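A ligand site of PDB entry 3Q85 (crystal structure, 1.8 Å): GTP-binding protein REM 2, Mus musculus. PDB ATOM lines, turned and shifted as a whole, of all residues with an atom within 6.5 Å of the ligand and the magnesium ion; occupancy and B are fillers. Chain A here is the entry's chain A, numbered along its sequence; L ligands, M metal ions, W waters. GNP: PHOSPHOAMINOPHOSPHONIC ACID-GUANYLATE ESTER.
Water W6 binds the magnesium ion, 2.1 Å away. Water W8 binds the magnesium ion (2.1 Å). O2G of the ligand binds the magnesium ion (2.2 Å). The side-chain hydroxyl (OG) of Ser 16 is bound to the magnesium ion (2.2 Å). The magnesium ion is bound by O2B of the ligand (2.4 Å). Water W10 is bound to the magnesium ion (2.4 Å).
One residue has an atom within 4 Å of the magnesium ion: Ser 16.
ND2 of Asn 117 sits at hydrogen-bond distance from O of Val 13 (2.9 Å). The backbone NH (N) of Ala 148 lies within hydrogen-bond range of the side-chain amide oxygen (OD1) of Asn 117 (3.0 Å). The backbone NH (N) of Ser 11 lies close to the side-chain amide nitrogen (NE2) of Gln 61, at 3.4 Å. O of Glu 10 sits at hydrogen-bond distance from NZ of Lys 15 (3.1 Å). OG of Ser 147 sits at hydrogen-bond distance from OD1 of Asp 120. The side-chain hydroxyl of Ser 147 lies within hydrogen-bond range of the backbone NH of Leu 150 (3.2 Å). N of Lys 118 is in hydrogen-bond range of O of Thr 146 (3.1 Å). OG1 of Thr 146 sits at hydrogen-bond distance from OD1 of Asn 117 (2.8 Å).
Water W9 lies within hydrogen-bond range of O3G of the ligand (2.8 Å), NE2 of Gln 61 (2.9 Å), O of Trp 59 (3.0 Å) and NZ of Lys 15 (3.4 Å).
Glu 10 touches the ligand. Leu 121 touches the ligand (CD2 to N2, 3.4 Å). Hydrophobic or aromatic side chains within 4 Å of the ligand: Val 13, Leu 121, Ala 148 and Ala 149. 15 residues have an atom within 4 Å of the ligand: Glu 10, Ser 11, Gly 12, Val 13, Gly 14, Lys 15, Ser 16, Thr 17, Asn 117, Lys 118, Asp 120, Leu 121, Ser 147, Ala 148 and Ala 149.
The side-chain amino group (NZ) of Lys 118 lies within hydrogen-bond range of an oxygen (O4') of the ligand (3.1 Å). N of Lys 118 sits close to O6 of the ligand, at 3.4 Å. O1G of the ligand is in hydrogen-bond range of OG of Ser 11 (2.6 Å). The backbone NH of Val 13 sits at hydrogen-bond distance from an oxygen (O1B) of the ligand (3.4 Å). The backbone NH (N) of Ala 149 lies within hydrogen-bond range of an oxygen (O6) of the ligand (3.2 Å). An oxygen (O1B) of the ligand sits at hydrogen-bond distance from the backbone NH (N) of Lys 15, at 3.1 Å. An oxygen (O1B) of the ligand is in hydrogen-bond range of the backbone NH (N) of Gly 14, 3.2 Å away. A nitrogen (N7) of the ligand is in hydrogen-bond range of the side-chain amide nitrogen of Asn 117, at 3.0 Å. O3G of the ligand is in salt-bridge range of NZ of Lys 15. An oxygen (O6) of the ligand is in hydrogen-bond range of the backbone NH (N) of Ala 148, 2.9 Å away. N1 of the ligand lies within hydrogen-bond range of OD1 of Asp 120 (2.7 Å). O1B of the ligand lies within hydrogen-bond range of N of Gly 12, 3.3 Å away. An oxygen (O2A) of the ligand lies within hydrogen-bond range of the side-chain hydroxyl (OG1) of Thr 17 (2.8 Å). An oxygen (O2A) of the ligand is in hydrogen-bond range of the backbone NH (N) of Thr 17, at 2.9 Å. An oxygen (O2A) of the ligand sits at hydrogen-bond distance from the backbone NH (N) of Ser 16 (3.2 Å). The side-chain hydroxyl (OG) of Ser 147 sits close to an oxygen (O6) of the ligand (3.4 Å).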
ATOM      1  N   GLY A   9      23.330  -7.677  22.752  1.00  0.00           N
ATOM      2  CA  GLY A   9      22.351  -6.600  22.679  1.00  0.00           C
ATOM      3  C   GLY A   9      22.579  -5.535  23.731  1.00  0.00           C
ATOM      4  O   GLY A   9      23.493  -5.646  24.554  1.00  0.00           O
ATOM      5  N   GLU A  10      21.760  -4.499  23.708  1.00  0.00           N
ATOM      6  CA  GLU A  10      21.960  -3.339  24.571  1.00  0.00           C
ATOM      7  C   GLU A  10      21.745  -3.699  26.043  1.00  0.00           C
ATOM      8  O   GLU A  10      21.088  -4.690  26.362  1.00  0.00           O
ATOM      9  CB  GLU A  10      21.002  -2.217  24.175  1.00  0.00           C
ATOM     10  CG  GLU A  10      21.215  -1.690  22.750  1.00  0.00           C
ATOM     11  CD  GLU A  10      22.598  -1.089  22.559  1.00  0.00           C
ATOM     12  OE1 GLU A  10      22.943  -0.133  23.295  1.00  0.00           O
ATOM     13  OE2 GLU A  10      23.350  -1.602  21.701  1.00  0.00           O
ATOM     14  N   SER A  11      22.304  -2.883  26.917  1.00  0.00           N
ATOM     15  CA  SER A  11      22.128  -3.059  28.354  1.00  0.00           C
ATOM     16  C   SER A  11      20.657  -2.983  28.730  1.00  0.00           C
ATOM     17  O   SER A  11      19.925  -2.154  28.216  1.00  0.00           O
ATOM     18  CB  SER A  11      22.906  -1.969  29.109  1.00  0.00           C
ATOM     19  OG  SER A  11      22.768  -2.133  30.510  1.00  0.00           O
ATOM     20  N   GLY A  12      20.219  -3.870  29.622  1.00  0.00           N
ATOM     21  CA  GLY A  12      18.901  -3.779  30.209  1.00  0.00           C
ATOM     22  C   GLY A  12      17.787  -4.529  29.476  1.00  0.00           C
ATOM     23  O   GLY A  12      16.678  -4.601  29.978  1.00  0.00           O
ATOM     24  N   VAL A  13      18.085  -5.077  28.305  1.00  0.00           N
ATOM     25  CA  VAL A  13      17.043  -5.696  27.490  1.00  0.00           C
ATOM     26  C   VAL A  13      16.559  -7.039  28.028  1.00  0.00           C
ATOM     27  O   VAL A  13      15.457  -7.464  27.713  1.00  0.00           O
ATOM     28  CB  VAL A  13      17.478  -5.908  26.027  1.00  0.00           C
ATOM     29  CG1 VAL A  13      17.842  -4.576  25.371  1.00  0.00           C
ATOM     30  CG2 VAL A  13      18.659  -6.891  25.943  1.00  0.00           C
ATOM     31  N   GLY A  14      17.400  -7.718  28.811  1.00  0.00           N
ATOM     32  CA  GLY A  14      17.017  -8.964  29.439  1.00  0.00           C
ATOM     33  C   GLY A  14      17.937 -10.141  29.146  1.00  0.00           C
ATOM     34  O   GLY A  14      17.545 -11.292  29.311  1.00  0.00           O
ATOM     35  N   LYS A  15      19.174  -9.866  28.728  1.00  0.00           N
ATOM     36  CA  LYS A  15      20.083 -10.941  28.321  1.00  0.00           C
ATOM     37  C   LYS A  15      20.349 -11.937  29.447  1.00  0.00           C
ATOM     38  O   LYS A  15      20.230 -13.149  29.266  1.00  0.00           O
ATOM     39  CB  LYS A  15      21.395 -10.354  27.789  1.00  0.00           C
ATOM     40  CG  LYS A  15      21.242  -9.590  26.480  1.00  0.00           C
ATOM     41  CD  LYS A  15      22.587  -9.155  25.903  1.00  0.00           C
ATOM     42  CE  LYS A  15      23.407  -8.344  26.897  1.00  0.00           C
ATOM     43  NZ  LYS A  15      22.721  -7.098  27.283  1.00  0.00           N
ATOM     44  N   SER A  16      20.714 -11.432  30.619  1.00  0.00           N
ATOM     45  CA  SER A  16      21.019 -12.294  31.748  1.00  0.00           C
ATOM     46  C   SER A  16      19.796 -13.048  32.252  1.00  0.00           C
ATOM     47  O   SER A  16      19.917 -14.156  32.730  1.00  0.00           O
ATOM     48  CB  SER A  16      21.613 -11.483  32.897  1.00  0.00           C
ATOM     49  OG  SER A  16      22.849 -10.958  32.493  1.00  0.00           O
ATOM     50  N   THR A  17      18.623 -12.432  32.143  1.00  0.00           N
ATOM     51  CA  THR A  17      17.414 -13.067  32.629  1.00  0.00           C
ATOM     52  C   THR A  17      17.090 -14.218  31.694  1.00  0.00           C
ATOM     53  O   THR A  17      16.722 -15.305  32.126  1.00  0.00           O
ATOM     54  CB  THR A  17      16.232 -12.056  32.726  1.00  0.00           C
ATOM     55  OG1 THR A  17      16.656 -10.904  33.466  1.00  0.00           O
ATOM     56  CG2 THR A  17      15.039 -12.675  33.426  1.00  0.00           C
ATOM     57  N   LEU A  18      17.279 -13.986  30.391  1.00  0.00           N
ATOM     58  CA  LEU A  18      17.093 -15.031  29.384  1.00  0.00           C
ATOM     59  C   LEU A  18      18.002 -16.214  29.650  1.00  0.00           C
ATOM     60  O   LEU A  18      17.581 -17.356  29.608  1.00  0.00           O
ATOM     61  CB  LEU A  18      17.363 -14.488  27.984  1.00  0.00           C
ATOM     62  CG  LEU A  18      16.237 -13.687  27.326  1.00  0.00           C
ATOM     63  CD1 LEU A  18      16.714 -13.099  25.993  1.00  0.00           C
ATOM     64  CD2 LEU A  18      15.012 -14.577  27.119  1.00  0.00           C
ATOM     65  N   ASP A  38      29.214 -16.744  33.769  1.00  0.00           N
ATOM     66  CA  ASP A  38      28.286 -16.195  32.790  1.00  0.00           C
ATOM     67  C   ASP A  38      28.194 -17.069  31.535  1.00  0.00           C
ATOM     68  O   ASP A  38      28.032 -16.575  30.418  1.00  0.00           O
ATOM     69  CB  ASP A  38      28.690 -14.766  32.438  1.00  0.00           C
ATOM     70  CG  ASP A  38      28.204 -13.760  33.460  1.00  0.00           C
ATOM     71  OD1 ASP A  38      28.452 -13.969  34.668  1.00  0.00           O
ATOM     72  OD2 ASP A  38      27.547 -12.773  33.065  1.00  0.00           O
ATOM     73  N   ASP A  57      26.545 -15.423  28.010  1.00  0.00           N
ATOM     74  CA  ASP A  57      26.023 -14.129  28.420  1.00  0.00           C
ATOM     75  C   ASP A  57      27.219 -13.264  28.809  1.00  0.00           C
ATOM     76  O   ASP A  57      27.396 -12.922  29.975  1.00  0.00           O
ATOM     77  CB  ASP A  57      25.052 -14.286  29.591  1.00  0.00           C
ATOM     78  CG  ASP A  57      24.522 -12.947  30.106  1.00  0.00           C
ATOM     79  OD1 ASP A  57      24.339 -12.021  29.295  1.00  0.00           O
ATOM     80  OD2 ASP A  57      24.293 -12.824  31.333  1.00  0.00           O
ATOM     81  N   TRP A  59      28.373 -10.577  26.581  1.00  0.00           N
ATOM     82  CA  TRP A  59      28.388  -9.423  25.692  1.00  0.00           C
ATOM     83  C   TRP A  59      28.526  -8.136  26.500  1.00  0.00           C
ATOM     84  O   TRP A  59      27.825  -7.946  27.493  1.00  0.00           O
ATOM     85  CB  TRP A  59      27.116  -9.376  24.861  1.00  0.00           C
ATOM     86  CG  TRP A  59      27.044  -8.221  23.915  1.00  0.00           C
ATOM     87  CD1 TRP A  59      26.367  -7.048  24.108  1.00  0.00           C
ATOM     88  CD2 TRP A  59      27.643  -8.133  22.615  1.00  0.00           C
ATOM     89  NE1 TRP A  59      26.520  -6.237  23.006  1.00  0.00           N
ATOM     90  CE2 TRP A  59      27.298  -6.877  22.085  1.00  0.00           C
ATOM     91  CE3 TRP A  59      28.455  -8.990  21.861  1.00  0.00           C
ATOM     92  CZ2 TRP A  59      27.730  -6.461  20.828  1.00  0.00           C
ATOM     93  CZ3 TRP A  59      28.870  -8.578  20.617  1.00  0.00           C
ATOM     94  CH2 TRP A  59      28.519  -7.322  20.109  1.00  0.00           C
ATOM     95  N   GLN A  61      29.244  -3.651  26.277  1.00  0.00           N
ATOM     96  CA  GLN A  61      28.944  -2.504  25.444  1.00  0.00           C
ATOM     97  C   GLN A  61      30.220  -1.812  24.972  1.00  0.00           C
ATOM     98  O   GLN A  61      31.175  -1.670  25.747  1.00  0.00           O
ATOM     99  CB  GLN A  61      28.074  -1.512  26.224  1.00  0.00           C
ATOM    100  CG  GLN A  61      26.834  -2.144  26.831  1.00  0.00           C
ATOM    101  CD  GLN A  61      25.932  -2.754  25.772  1.00  0.00           C
ATOM    102  OE1 GLN A  61      25.749  -2.182  24.696  1.00  0.00           O
ATOM    103  NE2 GLN A  61      25.381  -3.921  26.070  1.00  0.00           N
ATOM    104  N   ASN A 117      12.326  -9.067  23.754  1.00  0.00           N
ATOM    105  CA  ASN A 117      12.041  -9.495  25.118  1.00  0.00           C
ATOM    106  C   ASN A 117      11.120  -8.520  25.888  1.00  0.00           C
ATOM    107  O   ASN A 117      10.890  -7.403  25.446  1.00  0.00           O
ATOM    108  CB  ASN A 117      13.357  -9.653  25.891  1.00  0.00           C
ATOM    109  CG  ASN A 117      13.172 -10.347  27.222  1.00  0.00           C
ATOM    110  OD1 ASN A 117      12.458 -11.349  27.320  1.00  0.00           O
ATOM    111  ND2 ASN A 117      13.824  -9.821  28.256  1.00  0.00           N
ATOM    112  N   LYS A 118      10.629  -8.975  27.045  1.00  0.00           N
ATOM    113  CA  LYS A 118       9.703  -8.196  27.874  1.00  0.00           C
ATOM    114  C   LYS A 118       8.309  -8.060  27.260  1.00  0.00           C
ATOM    115  O   LYS A 118       7.627  -7.075  27.480  1.00  0.00           O
ATOM    116  CB  LYS A 118      10.279  -6.819  28.202  1.00  0.00           C
ATOM    117  CG  LYS A 118      11.692  -6.869  28.771  1.00  0.00           C
ATOM    118  CD  LYS A 118      12.034  -5.599  29.553  1.00  0.00           C
ATOM    119  CE  LYS A 118      13.506  -5.609  29.976  1.00  0.00           C
ATOM    120  NZ  LYS A 118      13.875  -4.445  30.853  1.00  0.00           N
ATOM    121  N   SER A 119       7.879  -9.064  26.504  1.00  0.00           N
ATOM    122  CA  SER A 119       6.572  -9.030  25.859  1.00  0.00           C
ATOM    123  C   SER A 119       5.421  -8.965  26.864  1.00  0.00           C
ATOM    124  O   SER A 119       4.282  -8.671  26.499  1.00  0.00           O
ATOM    125  CB  SER A 119       6.397 -10.263  24.984  1.00  0.00           C
ATOM    126  OG  SER A 119       6.376 -11.434  25.788  1.00  0.00           O
ATOM    127  N   ASP A 120       5.726  -9.268  28.115  1.00  0.00           N
ATOM    128  CA  ASP A 120       4.712  -9.297  29.168  1.00  0.00           C
ATOM    129  C   ASP A 120       4.287  -7.901  29.605  1.00  0.00           C
ATOM    130  O   ASP A 120       3.241  -7.742  30.231  1.00  0.00           O
ATOM    131  CB  ASP A 120       5.229 -10.099  30.375  1.00  0.00           C
ATOM    132  CG  ASP A 120       6.474  -9.476  31.000  1.00  0.00           C
ATOM    133  OD1 ASP A 120       7.588  -9.697  30.476  1.00  0.00           O
ATOM    134  OD2 ASP A 120       6.334  -8.789  32.040  1.00  0.00           O
ATOM    135  N   LEU A 121       5.089  -6.902  29.266  1.00  0.00           N
ATOM    136  CA  LEU A 121       4.820  -5.519  29.654  1.00  0.00           C
ATOM    137  C   LEU A 121       4.007  -4.782  28.582  1.00  0.00           C
ATOM    138  O   LEU A 121       4.505  -3.863  27.935  1.00  0.00           O
ATOM    139  CB  LEU A 121       6.146  -4.780  29.899  1.00  0.00           C
ATOM    140  CG  LEU A 121       7.007  -5.395  31.007  1.00  0.00           C
ATOM    141  CD1 LEU A 121       8.322  -4.627  31.175  1.00  0.00           C
ATOM    142  CD2 LEU A 121       6.238  -5.446  32.324  1.00  0.00           C
ATOM    143  N   THR A 146       9.750 -12.868  23.499  1.00  0.00           N
ATOM    144  CA  THR A 146       9.877 -13.648  24.712  1.00  0.00           C
ATOM    145  C   THR A 146       9.523 -12.823  25.934  1.00  0.00           C
ATOM    146  O   THR A 146       9.550 -11.594  25.903  1.00  0.00           O
ATOM    147  CB  THR A 146      11.332 -14.126  24.939  1.00  0.00           C
ATOM    148  OG1 THR A 146      12.202 -12.978  25.019  1.00  0.00           O
ATOM    149  CG2 THR A 146      11.791 -15.034  23.816  1.00  0.00           C
ATOM    150  N   SER A 147       9.208 -13.528  27.019  1.00  0.00           N
ATOM    151  CA  SER A 147       9.245 -12.928  28.341  1.00  0.00           C
ATOM    152  C   SER A 147      10.181 -13.758  29.183  1.00  0.00           C
ATOM    153  O   SER A 147       9.795 -14.820  29.680  1.00  0.00           O
ATOM    154  CB  SER A 147       7.870 -12.898  28.991  1.00  0.00           C
ATOM    155  OG  SER A 147       7.981 -12.401  30.324  1.00  0.00           O
ATOM    156  N   ALA A 148      11.406 -13.288  29.338  1.00  0.00           N
ATOM    157  CA  ALA A 148      12.375 -13.984  30.165  1.00  0.00           C
ATOM    158  C   ALA A 148      11.865 -14.073  31.597  1.00  0.00           C
ATOM    159  O   ALA A 148      12.167 -15.019  32.311  1.00  0.00           O
ATOM    160  CB  ALA A 148      13.710 -13.248  30.129  1.00  0.00           C
ATOM    161  N   ALA A 149      11.066 -13.092  32.025  1.00  0.00           N
ATOM    162  CA  ALA A 149      10.550 -13.063  33.390  1.00  0.00           C
ATOM    163  C   ALA A 149       9.564 -14.213  33.644  1.00  0.00           C
ATOM    164  O   ALA A 149       9.539 -14.788  34.723  1.00  0.00           O
ATOM    165  CB  ALA A 149       9.886 -11.727  33.685  1.00  0.00           C
ATOM    166  N   LEU A 150       8.749 -14.529  32.643  1.00  0.00           N
ATOM    167  CA  LEU A 150       7.727 -15.564  32.813  1.00  0.00           C
ATOM    168  C   LEU A 150       8.017 -16.820  31.995  1.00  0.00           C
ATOM    169  O   LEU A 150       7.172 -17.707  31.899  1.00  0.00           O
ATOM    170  CB  LEU A 150       6.364 -14.996  32.446  1.00  0.00           C
ATOM    171  CG  LEU A 150       6.065 -13.667  33.136  1.00  0.00           C
ATOM    172  CD1 LEU A 150       4.693 -13.180  32.748  1.00  0.00           C
ATOM    173  CD2 LEU A 150       6.192 -13.807  34.649  1.00  0.00           C
HETATM  174  PG  GNP L   1      23.183  -5.786  31.049  1.00  0.00           P
HETATM  175  O1G GNP L   1      23.499  -4.380  31.504  1.00  0.00           O
HETATM  176  O2G GNP L   1      23.936  -6.840  31.806  1.00  0.00           O
HETATM  177  O3G GNP L   1      23.479  -5.761  29.585  1.00  0.00           O
HETATM  178  N3B GNP L   1      21.618  -6.068  31.283  1.00  0.00           N
HETATM  179  PB  GNP L   1      20.783  -7.301  30.696  1.00  0.00           P
HETATM  180  O1B GNP L   1      20.562  -7.152  29.250  1.00  0.00           O
HETATM  181  O2B GNP L   1      21.431  -8.553  31.126  1.00  0.00           O
HETATM  182  O3A GNP L   1      19.395  -7.283  31.370  1.00  0.00           O
HETATM  183  PA  GNP L   1      18.941  -8.078  32.597  1.00  0.00           P
HETATM  184  O1A GNP L   1      19.837  -7.774  33.732  1.00  0.00           O
HETATM  185  O2A GNP L   1      18.714  -9.497  32.255  1.00  0.00           O
HETATM  186  O5' GNP L   1      17.511  -7.549  32.977  1.00  0.00           O
HETATM  187  C5' GNP L   1      17.312  -6.157  33.171  1.00  0.00           C
HETATM  188  C4' GNP L   1      16.041  -5.923  33.952  1.00  0.00           C
HETATM  189  O4' GNP L   1      14.882  -6.273  33.152  1.00  0.00           O
HETATM  190  C3' GNP L   1      15.929  -6.732  35.238  1.00  0.00           C
HETATM  191  O3' GNP L   1      15.413  -5.905  36.266  1.00  0.00           O
HETATM  192  C2' GNP L   1      14.980  -7.867  34.853  1.00  0.00           C
HETATM  193  O2' GNP L   1      14.218  -8.383  35.938  1.00  0.00           O
HETATM  194  C1' GNP L   1      14.053  -7.183  33.855  1.00  0.00           C
HETATM  195  N9  GNP L   1      13.525  -8.101  32.859  1.00  0.00           N
HETATM  196  C8  GNP L   1      14.260  -8.937  32.051  1.00  0.00           C
HETATM  197  N7  GNP L   1      13.532  -9.655  31.250  1.00  0.00           N
HETATM  198  C5  GNP L   1      12.232  -9.265  31.541  1.00  0.00           C
HETATM  199  C6  GNP L   1      11.015  -9.692  30.979  1.00  0.00           C
HETATM  200  O6  GNP L   1      10.835 -10.534  30.090  1.00  0.00           O
HETATM  201  N1  GNP L   1       9.921  -9.038  31.547  1.00  0.00           N
HETATM  202  C2  GNP L   1      10.004  -8.094  32.548  1.00  0.00           C
HETATM  203  N2  GNP L   1       8.841  -7.574  32.975  1.00  0.00           N
HETATM  204  N3  GNP L   1      11.146  -7.675  33.079  1.00  0.00           N
HETATM  205  C4  GNP L   1      12.214  -8.304  32.523  1.00  0.00           C
HETATM  206 MG    MG M   1      23.568  -8.942  32.083  1.00  0.00          MG
HETATM  207  O   HOH W   1      12.773  -6.503  37.660  1.00  0.00           O
HETATM  208  O   HOH W   2      18.006  -2.804  33.658  1.00  0.00           O
HETATM  209  O   HOH W   3      20.423  -4.538  33.561  1.00  0.00           O
HETATM  210  O   HOH W   4       8.355  -6.296  35.592  1.00  0.00           O
HETATM  211  O   HOH W   5      19.308  -9.383  36.594  1.00  0.00           O
HETATM  212  O   HOH W   6      25.297  -9.134  33.237  1.00  0.00           O
HETATM  213  O   HOH W   7      12.462 -10.552  35.364  1.00  0.00           O
HETATM  214  O   HOH W   8      24.330  -9.579  30.205  1.00  0.00           O
HETATM  215  O   HOH W   9      25.795  -5.885  28.104  1.00  0.00           O
HETATM  216  O   HOH W  10      22.347  -8.423  34.059  1.00  0.00           O
HETATM  217  O   HOH W  11      26.943  -6.803  31.787  1.00  0.00           O
